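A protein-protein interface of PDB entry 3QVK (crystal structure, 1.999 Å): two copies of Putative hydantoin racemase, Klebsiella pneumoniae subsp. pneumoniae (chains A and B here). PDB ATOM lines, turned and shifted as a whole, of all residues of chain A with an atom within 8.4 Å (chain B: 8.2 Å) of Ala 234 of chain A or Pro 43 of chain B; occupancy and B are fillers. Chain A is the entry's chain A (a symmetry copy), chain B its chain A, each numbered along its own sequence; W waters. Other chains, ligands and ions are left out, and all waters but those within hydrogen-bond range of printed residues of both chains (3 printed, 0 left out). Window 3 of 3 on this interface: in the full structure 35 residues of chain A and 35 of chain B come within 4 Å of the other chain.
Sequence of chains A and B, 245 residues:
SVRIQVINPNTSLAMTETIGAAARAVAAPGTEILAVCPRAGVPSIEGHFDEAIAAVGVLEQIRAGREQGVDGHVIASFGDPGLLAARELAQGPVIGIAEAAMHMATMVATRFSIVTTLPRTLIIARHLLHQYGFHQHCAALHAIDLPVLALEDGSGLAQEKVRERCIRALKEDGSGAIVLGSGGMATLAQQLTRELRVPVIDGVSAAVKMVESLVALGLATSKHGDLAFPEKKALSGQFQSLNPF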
ATOM      1  N   GLU A 231      14.544  12.595  30.730  1.00  0.00           N
ATOM      2  CA  GLU A 231      13.268  12.903  31.375  1.00  0.00           C
ATOM      3  C   GLU A 231      12.295  13.473  30.348  1.00  0.00           C
ATOM      4  O   GLU A 231      12.693  14.248  29.476  1.00  0.00           O
ATOM      5  CB  GLU A 231      13.459  13.898  32.526  1.00  0.00           C
ATOM      6  CG  GLU A 231      14.476  13.475  33.590  1.00  0.00           C
ATOM      7  CD  GLU A 231      14.062  12.232  34.367  1.00  0.00           C
ATOM      8  OE1 GLU A 231      12.863  12.093  34.694  1.00  0.00           O
ATOM      9  OE2 GLU A 231      14.944  11.398  34.657  1.00  0.00           O
ATOM     10  N   LYS A 232      11.029  13.070  30.446  1.00  0.00           N
ATOM     11  CA  LYS A 232      10.008  13.507  29.495  1.00  0.00           C
ATOM     12  C   LYS A 232       9.764  15.011  29.585  1.00  0.00           C
ATOM     13  O   LYS A 232       9.303  15.520  30.610  1.00  0.00           O
ATOM     14  CB  LYS A 232       8.697  12.740  29.697  1.00  0.00           C
ATOM     15  CG  LYS A 232       7.622  13.109  28.682  1.00  0.00           C
ATOM     16  CD  LYS A 232       6.282  12.473  29.005  1.00  0.00           C
ATOM     17  CE  LYS A 232       5.184  13.028  28.105  1.00  0.00           C
ATOM     18  NZ  LYS A 232       5.447  12.773  26.659  1.00  0.00           N
ATOM     19  N   LYS A 233      10.092  15.711  28.502  1.00  0.00           N
ATOM     20  CA  LYS A 233       9.869  17.152  28.398  1.00  0.00           C
ATOM     21  C   LYS A 233       9.796  17.600  26.941  1.00  0.00           C
ATOM     22  O   LYS A 233      10.283  16.910  26.043  1.00  0.00           O
ATOM     23  CB  LYS A 233      10.940  17.941  29.166  1.00  0.00           C
ATOM     24  CG  LYS A 233      12.377  17.622  28.783  1.00  0.00           C
ATOM     25  CD  LYS A 233      13.363  18.223  29.775  1.00  0.00           C
ATOM     26  CE  LYS A 233      13.551  17.353  31.006  1.00  0.00           C
ATOM     27  NZ  LYS A 233      14.631  17.891  31.878  1.00  0.00           N
ATOM     28  N   ALA A 234       9.185  18.760  26.720  1.00  0.00           N
ATOM     29  CA  ALA A 234       8.958  19.274  25.376  1.00  0.00           C
ATOM     30  C   ALA A 234      10.150  20.067  24.854  1.00  0.00           C
ATOM     31  O   ALA A 234      10.553  21.070  25.445  1.00  0.00           O
ATOM     32  CB  ALA A 234       7.708  20.123  25.353  1.00  0.00           C
ATOM     33  N   LEU A 235      10.707  19.603  23.739  1.00  0.00           N
ATOM     34  CA  LEU A 235      11.815  20.285  23.081  1.00  0.00           C
ATOM     35  C   LEU A 235      11.268  21.255  22.035  1.00  0.00           C
ATOM     36  O   LEU A 235      10.333  20.925  21.304  1.00  0.00           O
ATOM     37  CB  LEU A 235      12.769  19.268  22.445  1.00  0.00           C
ATOM     38  CG  LEU A 235      13.275  18.133  23.348  1.00  0.00           C
ATOM     39  CD1 LEU A 235      14.061  17.102  22.553  1.00  0.00           C
ATOM     40  CD2 LEU A 235      14.107  18.662  24.512  1.00  0.00           C
ATOM     41  N   SER A 236      11.849  22.451  21.977  1.00  0.00           N
ATOM     42  CA  SER A 236      11.346  23.505  21.096  1.00  0.00           C
ATOM     43  C   SER A 236      12.263  23.794  19.910  1.00  0.00           C
ATOM     44  O   SER A 236      13.467  23.527  19.960  1.00  0.00           O
ATOM     45  CB  SER A 236      11.086  24.790  21.888  1.00  0.00           C
ATOM     46  OG  SER A 236      12.272  25.262  22.504  1.00  0.00           O
ATOM     47  N   GLY A 237      11.670  24.331  18.846  1.00  0.00           N
ATOM     48  CA  GLY A 237      12.400  24.763  17.657  1.00  0.00           C
ATOM     49  C   GLY A 237      13.160  23.662  16.944  1.00  0.00           C
ATOM     50  O   GLY A 237      12.600  22.618  16.611  1.00  0.00           O
ATOM     51  N   PHE A 239      15.233  21.559  17.961  1.00  0.00           N
ATOM     52  CA  PHE A 239      15.496  20.356  18.756  1.00  0.00           C
ATOM     53  C   PHE A 239      14.278  19.442  18.940  1.00  0.00           C
ATOM     54  O   PHE A 239      14.403  18.353  19.502  1.00  0.00           O
ATOM     55  CB  PHE A 239      16.060  20.736  20.130  1.00  0.00           C
ATOM     56  CG  PHE A 239      17.253  21.652  20.071  1.00  0.00           C
ATOM     57  CD1 PHE A 239      18.504  21.172  19.694  1.00  0.00           C
ATOM     58  CD2 PHE A 239      17.125  22.996  20.407  1.00  0.00           C
ATOM     59  CE1 PHE A 239      19.609  22.019  19.642  1.00  0.00           C
ATOM     60  CE2 PHE A 239      18.225  23.852  20.364  1.00  0.00           C
ATOM     61  CZ  PHE A 239      19.467  23.362  19.976  1.00  0.00           C
ATOM     62  N   GLN A 240      13.114  19.880  18.462  1.00  0.00           N
ATOM     63  CA  GLN A 240      11.850  19.172  18.713  1.00  0.00           C
ATOM     64  C   GLN A 240      11.799  17.730  18.187  1.00  0.00           C
ATOM     65  O   GLN A 240      11.037  16.907  18.700  1.00  0.00           O
ATOM     66  CB  GLN A 240      10.650  19.984  18.201  1.00  0.00           C
ATOM     67  CG  GLN A 240      10.564  20.149  16.685  1.00  0.00           C
ATOM     68  CD  GLN A 240       9.519  21.173  16.260  1.00  0.00           C
ATOM     69  OE1 GLN A 240       9.771  22.002  15.385  1.00  0.00           O
ATOM     70  NE2 GLN A 240       8.345  21.121  16.883  1.00  0.00           N
ATOM     71  N   ASN A 243      13.754  13.817  20.344  1.00  0.00           N
ATOM     72  CA  ASN A 243      13.195  12.801  21.236  1.00  0.00           C
ATOM     73  C   ASN A 243      11.692  12.565  21.017  1.00  0.00           C
ATOM     74  O   ASN A 243      10.866  13.057  21.791  1.00  0.00           O
ATOM     75  CB  ASN A 243      13.495  13.151  22.702  1.00  0.00           C
ATOM     76  CG  ASN A 243      13.300  11.974  23.649  1.00  0.00           C
ATOM     77  OD1 ASN A 243      13.258  10.815  23.229  1.00  0.00           O
ATOM     78  ND2 ASN A 243      13.188  12.271  24.938  1.00  0.00           N
ATOM     79  N   ASN B   8      20.574  31.992  30.907  1.00  0.00           N
ATOM     80  CA  ASN B   8      19.931  30.781  31.392  1.00  0.00           C
ATOM     81  C   ASN B   8      19.916  29.783  30.234  1.00  0.00           C
ATOM     82  O   ASN B   8      19.275  30.039  29.216  1.00  0.00           O
ATOM     83  CB  ASN B   8      18.508  31.082  31.884  1.00  0.00           C
ATOM     84  CG  ASN B   8      17.774  29.840  32.378  1.00  0.00           C
ATOM     85  OD1 ASN B   8      18.385  28.814  32.679  1.00  0.00           O
ATOM     86  ND2 ASN B   8      16.451  29.935  32.469  1.00  0.00           N
ATOM     87  N   PRO B   9      20.647  28.657  30.373  1.00  0.00           N
ATOM     88  CA  PRO B   9      20.782  27.678  29.291  1.00  0.00           C
ATOM     89  C   PRO B   9      19.495  26.913  28.982  1.00  0.00           C
ATOM     90  O   PRO B   9      19.371  26.347  27.894  1.00  0.00           O
ATOM     91  CB  PRO B   9      21.856  26.717  29.819  1.00  0.00           C
ATOM     92  CG  PRO B   9      22.565  27.487  30.880  1.00  0.00           C
ATOM     93  CD  PRO B   9      21.490  28.293  31.523  1.00  0.00           C
ATOM     94  N   ASN B  10      18.560  26.887  29.930  1.00  0.00           N
ATOM     95  CA  ASN B  10      17.238  26.317  29.677  1.00  0.00           C
ATOM     96  C   ASN B  10      16.237  27.384  29.214  1.00  0.00           C
ATOM     97  O   ASN B  10      16.495  28.581  29.355  1.00  0.00           O
ATOM     98  CB  ASN B  10      16.725  25.513  30.886  1.00  0.00           C
ATOM     99  CG  ASN B  10      16.351  26.385  32.076  1.00  0.00           C
ATOM    100  OD1 ASN B  10      15.523  27.290  31.969  1.00  0.00           O
ATOM    101  ND2 ASN B  10      16.940  26.090  33.229  1.00  0.00           N
ATOM    102  N   THR B  11      15.105  26.944  28.667  1.00  0.00           N
ATOM    103  CA  THR B  11      14.127  27.853  28.059  1.00  0.00           C
ATOM    104  C   THR B  11      13.028  28.325  29.019  1.00  0.00           C
ATOM    105  O   THR B  11      12.059  28.959  28.593  1.00  0.00           O
ATOM    106  CB  THR B  11      13.465  27.224  26.809  1.00  0.00           C
ATOM    107  OG1 THR B  11      12.782  26.022  27.182  1.00  0.00           O
ATOM    108  CG2 THR B  11      14.504  26.910  25.738  1.00  0.00           C
ATOM    109  N   SER B  12      13.175  28.017  30.305  1.00  0.00           N
ATOM    110  CA  SER B  12      12.211  28.458  31.314  1.00  0.00           C
ATOM    111  C   SER B  12      12.373  29.945  31.608  1.00  0.00           C
ATOM    112  O   SER B  12      13.387  30.370  32.170  1.00  0.00           O
ATOM    113  CB  SER B  12      12.360  27.643  32.600  1.00  0.00           C
ATOM    114  OG  SER B  12      11.599  28.207  33.658  1.00  0.00           O
ATOM    115  N   LEU B  13      11.369  30.732  31.228  1.00  0.00           N
ATOM    116  CA  LEU B  13      11.388  32.173  31.478  1.00  0.00           C
ATOM    117  C   LEU B  13      11.264  32.476  32.971  1.00  0.00           C
ATOM    118  O   LEU B  13      11.805  33.473  33.450  1.00  0.00           O
ATOM    119  CB  LEU B  13      10.287  32.887  30.687  1.00  0.00           C
ATOM    120  CG  LEU B  13      10.510  34.379  30.408  1.00  0.00           C
ATOM    121  CD1 LEU B  13      11.540  34.595  29.304  1.00  0.00           C
ATOM    122  CD2 LEU B  13       9.206  35.047  30.036  1.00  0.00           C
ATOM    123  N   ALA B  14      10.558  31.606  33.693  1.00  0.00           N
ATOM    124  CA  ALA B  14      10.430  31.704  35.147  1.00  0.00           C
ATOM    125  C   ALA B  14      11.789  31.600  35.841  1.00  0.00           C
ATOM    126  O   ALA B  14      12.088  32.376  36.752  1.00  0.00           O
ATOM    127  CB  ALA B  14       9.480  30.634  35.672  1.00  0.00           C
ATOM    128  N   MET B  15      12.604  30.642  35.403  1.00  0.00           N
ATOM    129  CA  MET B  15      13.950  30.463  35.940  1.00  0.00           C
ATOM    130  C   MET B  15      14.870  31.604  35.498  1.00  0.00           C
ATOM    131  O   MET B  15      15.735  32.037  36.261  1.00  0.00           O
ATOM    132  CB  MET B  15      14.523  29.099  35.536  1.00  0.00           C
ATOM    133  CG  MET B  15      15.703  28.634  36.388  1.00  0.00           C
ATOM    134  SD  MET B  15      15.862  26.835  36.481  1.00  0.00           S
ATOM    135  CE  MET B  15      14.580  26.439  37.667  1.00  0.00           C
ATOM    136  N   THR B  16      14.663  32.091  34.274  1.00  0.00           N
ATOM    137  CA  THR B  16      15.396  33.243  33.738  1.00  0.00           C
ATOM    138  C   THR B  16      15.169  34.499  34.589  1.00  0.00           C
ATOM    139  O   THR B  16      16.097  35.288  34.799  1.00  0.00           O
ATOM    140  CB  THR B  16      15.017  33.523  32.259  1.00  0.00           C
ATOM    141  OG1 THR B  16      15.118  32.314  31.496  1.00  0.00           O
ATOM    142  CG2 THR B  16      15.936  34.576  31.641  1.00  0.00           C
ATOM    143  N   ALA B  40      15.259  28.377  21.303  1.00  0.00           N
ATOM    144  CA  ALA B  40      14.932  26.964  21.148  1.00  0.00           C
ATOM    145  C   ALA B  40      15.759  26.118  22.109  1.00  0.00           C
ATOM    146  O   ALA B  40      16.938  26.399  22.341  1.00  0.00           O
ATOM    147  CB  ALA B  40      15.172  26.522  19.712  1.00  0.00           C
ATOM    148  N   GLY B  41      15.137  25.084  22.669  1.00  0.00           N
ATOM    149  CA  GLY B  41      15.844  24.172  23.560  1.00  0.00           C
ATOM    150  C   GLY B  41      14.965  23.395  24.516  1.00  0.00           C
ATOM    151  O   GLY B  41      13.899  22.900  24.145  1.00  0.00           O
ATOM    152  N   VAL B  42      15.429  23.304  25.759  1.00  0.00           N
ATOM    153  CA  VAL B  42      14.820  22.458  26.779  1.00  0.00           C
ATOM    154  C   VAL B  42      14.410  23.306  27.999  1.00  0.00           C
ATOM    155  O   VAL B  42      15.153  24.202  28.397  1.00  0.00           O
ATOM    156  CB  VAL B  42      15.794  21.290  27.152  1.00  0.00           C
ATOM    157  CG1 VAL B  42      17.028  21.791  27.912  1.00  0.00           C
ATOM    158  CG2 VAL B  42      15.085  20.195  27.910  1.00  0.00           C
ATOM    159  N   PRO B  43      13.212  23.049  28.571  1.00  0.00           N
ATOM    160  CA  PRO B  43      12.718  23.828  29.720  1.00  0.00           C
ATOM    161  C   PRO B  43      13.537  23.672  31.004  1.00  0.00           C
ATOM    162  O   PRO B  43      13.604  24.608  31.804  1.00  0.00           O
ATOM    163  CB  PRO B  43      11.299  23.285  29.928  1.00  0.00           C
ATOM    164  CG  PRO B  43      10.913  22.724  28.610  1.00  0.00           C
ATOM    165  CD  PRO B  43      12.174  22.136  28.061  1.00  0.00           C
ATOM    166  N   SER B  44      14.131  22.498  31.204  1.00  0.00           N
ATOM    167  CA  SER B  44      15.015  22.254  32.345  1.00  0.00           C
ATOM    168  C   SER B  44      16.100  21.253  31.969  1.00  0.00           C
ATOM    169  O   SER B  44      15.905  20.417  31.085  1.00  0.00           O
ATOM    170  CB  SER B  44      14.227  21.765  33.565  1.00  0.00           C
ATOM    171  OG  SER B  44      13.670  20.481  33.345  1.00  0.00           O
ATOM    172  N   ILE B  45      17.242  21.349  32.643  1.00  0.00           N
ATOM    173  CA  ILE B  45      18.388  20.497  32.342  1.00  0.00           C
ATOM    174  C   ILE B  45      18.563  19.438  33.430  1.00  0.00           C
ATOM    175  O   ILE B  45      18.925  19.751  34.568  1.00  0.00           O
ATOM    176  CB  ILE B  45      19.678  21.326  32.147  1.00  0.00           C
ATOM    177  CG1 ILE B  45      19.464  22.397  31.073  1.00  0.00           C
ATOM    178  CG2 ILE B  45      20.841  20.420  31.765  1.00  0.00           C
ATOM    179  CD1 ILE B  45      20.344  23.624  31.231  1.00  0.00           C
ATOM    180  N   GLU B  46      18.288  18.187  33.063  1.00  0.00           N
ATOM    181  CA  GLU B  46      18.272  17.071  34.008  1.00  0.00           C
ATOM    182  C   GLU B  46      18.969  15.842  33.426  1.00  0.00           C
ATOM    183  O   GLU B  46      18.403  14.746  33.404  1.00  0.00           O
ATOM    184  CB  GLU B  46      16.828  16.723  34.394  1.00  0.00           C
ATOM    185  CG  GLU B  46      16.053  17.862  35.046  1.00  0.00           C
ATOM    186  CD  GLU B  46      14.585  17.541  35.256  1.00  0.00           C
ATOM    187  OE1 GLU B  46      13.962  16.929  34.362  1.00  0.00           O
ATOM    188  OE2 GLU B  46      14.051  17.915  36.318  1.00  0.00           O
ATOM    189  N   ASP B  50      19.956  16.698  27.868  1.00  0.00           N
ATOM    190  CA  ASP B  50      19.510  18.076  28.081  1.00  0.00           C
ATOM    191  C   ASP B  50      20.664  19.076  27.981  1.00  0.00           C
ATOM    192  O   ASP B  50      20.494  20.169  27.439  1.00  0.00           O
ATOM    193  CB  ASP B  50      18.815  18.216  29.440  1.00  0.00           C
ATOM    194  CG  ASP B  50      17.531  17.399  29.543  1.00  0.00           C
ATOM    195  OD1 ASP B  50      16.975  16.990  28.500  1.00  0.00           O
ATOM    196  OD2 ASP B  50      17.074  17.173  30.682  1.00  0.00           O
ATOM    197  N   ILE B  53      21.812  19.852  24.317  1.00  0.00           N
ATOM    198  CA  ILE B  53      20.868  20.794  23.720  1.00  0.00           C
ATOM    199  C   ILE B  53      21.108  22.205  24.267  1.00  0.00           C
ATOM    200  O   ILE B  53      21.159  23.172  23.501  1.00  0.00           O
ATOM    201  CB  ILE B  53      19.399  20.359  23.961  1.00  0.00           C
ATOM    202  CG1 ILE B  53      19.110  19.038  23.240  1.00  0.00           C
ATOM    203  CG2 ILE B  53      18.426  21.440  23.497  1.00  0.00           C
ATOM    204  CD1 ILE B  53      17.815  18.374  23.659  1.00  0.00           C
ATOM    205  N   VAL B 148      14.104  19.854  38.680  1.00  0.00           N
ATOM    206  CA  VAL B 148      14.682  21.204  38.712  1.00  0.00           C
ATOM    207  C   VAL B 148      13.622  22.300  38.884  1.00  0.00           C
ATOM    208  O   VAL B 148      13.790  23.215  39.695  1.00  0.00           O
ATOM    209  CB  VAL B 148      15.556  21.471  37.451  1.00  0.00           C
ATOM    210  CG1 VAL B 148      15.995  22.930  37.379  1.00  0.00           C
ATOM    211  CG2 VAL B 148      16.775  20.559  37.448  1.00  0.00           C
ATOM    212  N   LEU B 149      12.523  22.181  38.141  1.00  0.00           N
ATOM    213  CA  LEU B 149      11.476  23.207  38.123  1.00  0.00           C
ATOM    214  C   LEU B 149      10.573  23.218  39.365  1.00  0.00           C
ATOM    215  O   LEU B 149       9.693  24.074  39.484  1.00  0.00           O
ATOM    216  CB  LEU B 149      10.641  23.102  36.838  1.00  0.00           C
ATOM    217  CG  LEU B 149      11.387  23.301  35.512  1.00  0.00           C
ATOM    218  CD1 LEU B 149      10.481  22.992  34.332  1.00  0.00           C
ATOM    219  CD2 LEU B 149      11.973  24.706  35.390  1.00  0.00           C
HETATM  220  O   HOH W   1      16.816  14.441  31.196  1.00  0.00           O
HETATM  221  O   HOH W   2      11.663  24.785  25.179  1.00  0.00           O
HETATM  222  O   HOH W   3      14.738  15.490  27.877  1.00  0.00           O
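Among the printed residues, merely in contact across the chains: Glu 231 of chain A with Glu 46 of chain B (3.6 Å), Lys 233 of chain A with Val 42 of chain B (3.2 Å), Ala 234 of chain A with Pro 43 of chain B (3.3 Å), Leu 235 of chain A with Gly 41 of chain B (3.5 Å), Leu 235 of chain A with Val 42 of chain B (3.9 Å), Leu 235 of chain A with Ile 53 of chain B (3.8 Å), Ser 236 of chain A with Ala 40 of chain B (3.4 Å), Gly 237 of chain A with Ala 40 of chain B (3.9 Å), Phe 239 of chain A with Ala 40 of chain B (3.5 Å), Phe 239 of chain A with Gly 41 of chain B (3.6 Å) and Phe 239 of chain A with Ile 53 of chain B (3.6 Å).
The backbone NH (N) of Gly 41 of chain B sits at hydrogen-bond distance from the side-chain hydroxyl (OG) of Ser 236 of chain A.
The backbone carbonyl oxygen (O) of Ser 44 of chain B is in hydrogen-bond range of the side-chain amino group (NZ) of Lys 233 of chain A (2.9 Å).
The side-chain carboxylate (OE1) of Glu 46 of chain B is in salt-bridge range of the side-chain amino group (NZ) of Lys 233 of chain A, at 2.7 Å.
The side-chain amino group (NZ) of Lys 233 of chain A is in salt-bridge range of the side-chain carboxylate (OD2) of Asp 50 of chain B (2.8 Å).
No position is printed for both chains.
Printed residues of chain A that touch a printed residue of chain B: Glu 231, Lys 233, Ala 234, Leu 235, Ser 236, Gly 237 and Phe 239.
Hydrophobic or aromatic side chains of chain A that line the printed part of chain B: Leu 235 and Phe 239.
Of the 20 printed residues of chain B, 8 touch a printed residue of chain A.
Hydrophobic or aromatic side chains of chain B that line the printed part of chain A: Ala 40, Val 42, Pro 43 and Ile 53.
Among the printed residues, 15 pairs touch across the chains.
Among the printed residues, Asp or Glu carboxylates within 4 Å of a Lys or Arg side-chain nitrogen of the other chain: Lys 233 of chain A with Glu 46 of chain B (2.7 Å) and Lys 233 of chain A with Asp 50 of chain B (2.8 Å).
Water W2 lies within hydrogen-bond range of the side-chain hydroxyl of Thr 11 of chain B (2.6 Å), the side-chain hydroxyl of Ser 236 of chain A (2.8 Å) and the backbone carbonyl oxygen of Gly 41 of chain B (3.1 Å).
Water W1 lies within hydrogen-bond range of the backbone carbonyl oxygen (O) of Glu 46 of chain B (2.7 Å), the side-chain carboxylate (OD2) of Asp 50 of chain B (2.8 Å) and the backbone NH (N) of Glu 231 of chain A (3.0 Å).
Water W3 lies within hydrogen-bond range of the side-chain carboxylate (OD1) of Asp 50 of chain B and the backbone carbonyl oxygen (O) of Glu 231 of chain A.
Lys 232 of chain A touches none of the printed residues of chain B.
Of the printed residues of chain B, Lys 233 of chain A touches Val 42, Ser 44, Glu 46 and Asp 50.
Of chain B, only Pro 43 (3.3 Å) comes within 4 Å of Ala 234 of chain A.
Of the printed residues of chain B, Leu 235 of chain A touches Gly 41, Val 42 and Ile 53.
Of the printed residues of chain B, Ser 236 of chain A touches Ala 40 and Gly 41.
Of the printed residues of chain B, Phe 239 of chain A touches Ala 40 (3.5 Å), Gly 41 (3.6 Å) and Ile 53 (3.6 Å).
Of chain A, only Ala 234 (3.3 Å) comes within 4 Å of Pro 43 of chain B.
Printed residues of chain A within 4 Å of Asp 50 of chain B: Lys 233 (2.8 Å).
The side-chain amide oxygen of Asn 10 of chain B lies close to the backbone carbonyl oxygen of Pro 43 of chain B.
The backbone carbonyl oxygen (O) of Val 42 of chain B is in hydrogen-bond range of the backbone NH (N) of Thr 11 of chain B (2.8 Å).
The side-chain carboxylate of Asp 50 of chain B sits at hydrogen-bond distance from the backbone NH of Glu 46 of chain B (2.9 Å).
The backbone NH of Val 148 of chain B sits at hydrogen-bond distance from the side-chain carboxylate of Glu 46 of chain B (3.1 Å).
The side-chain amide oxygen of Gln 240 of chain A lies close to the backbone carbonyl oxygen of Gly 237 of chain A (3.1 Å).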
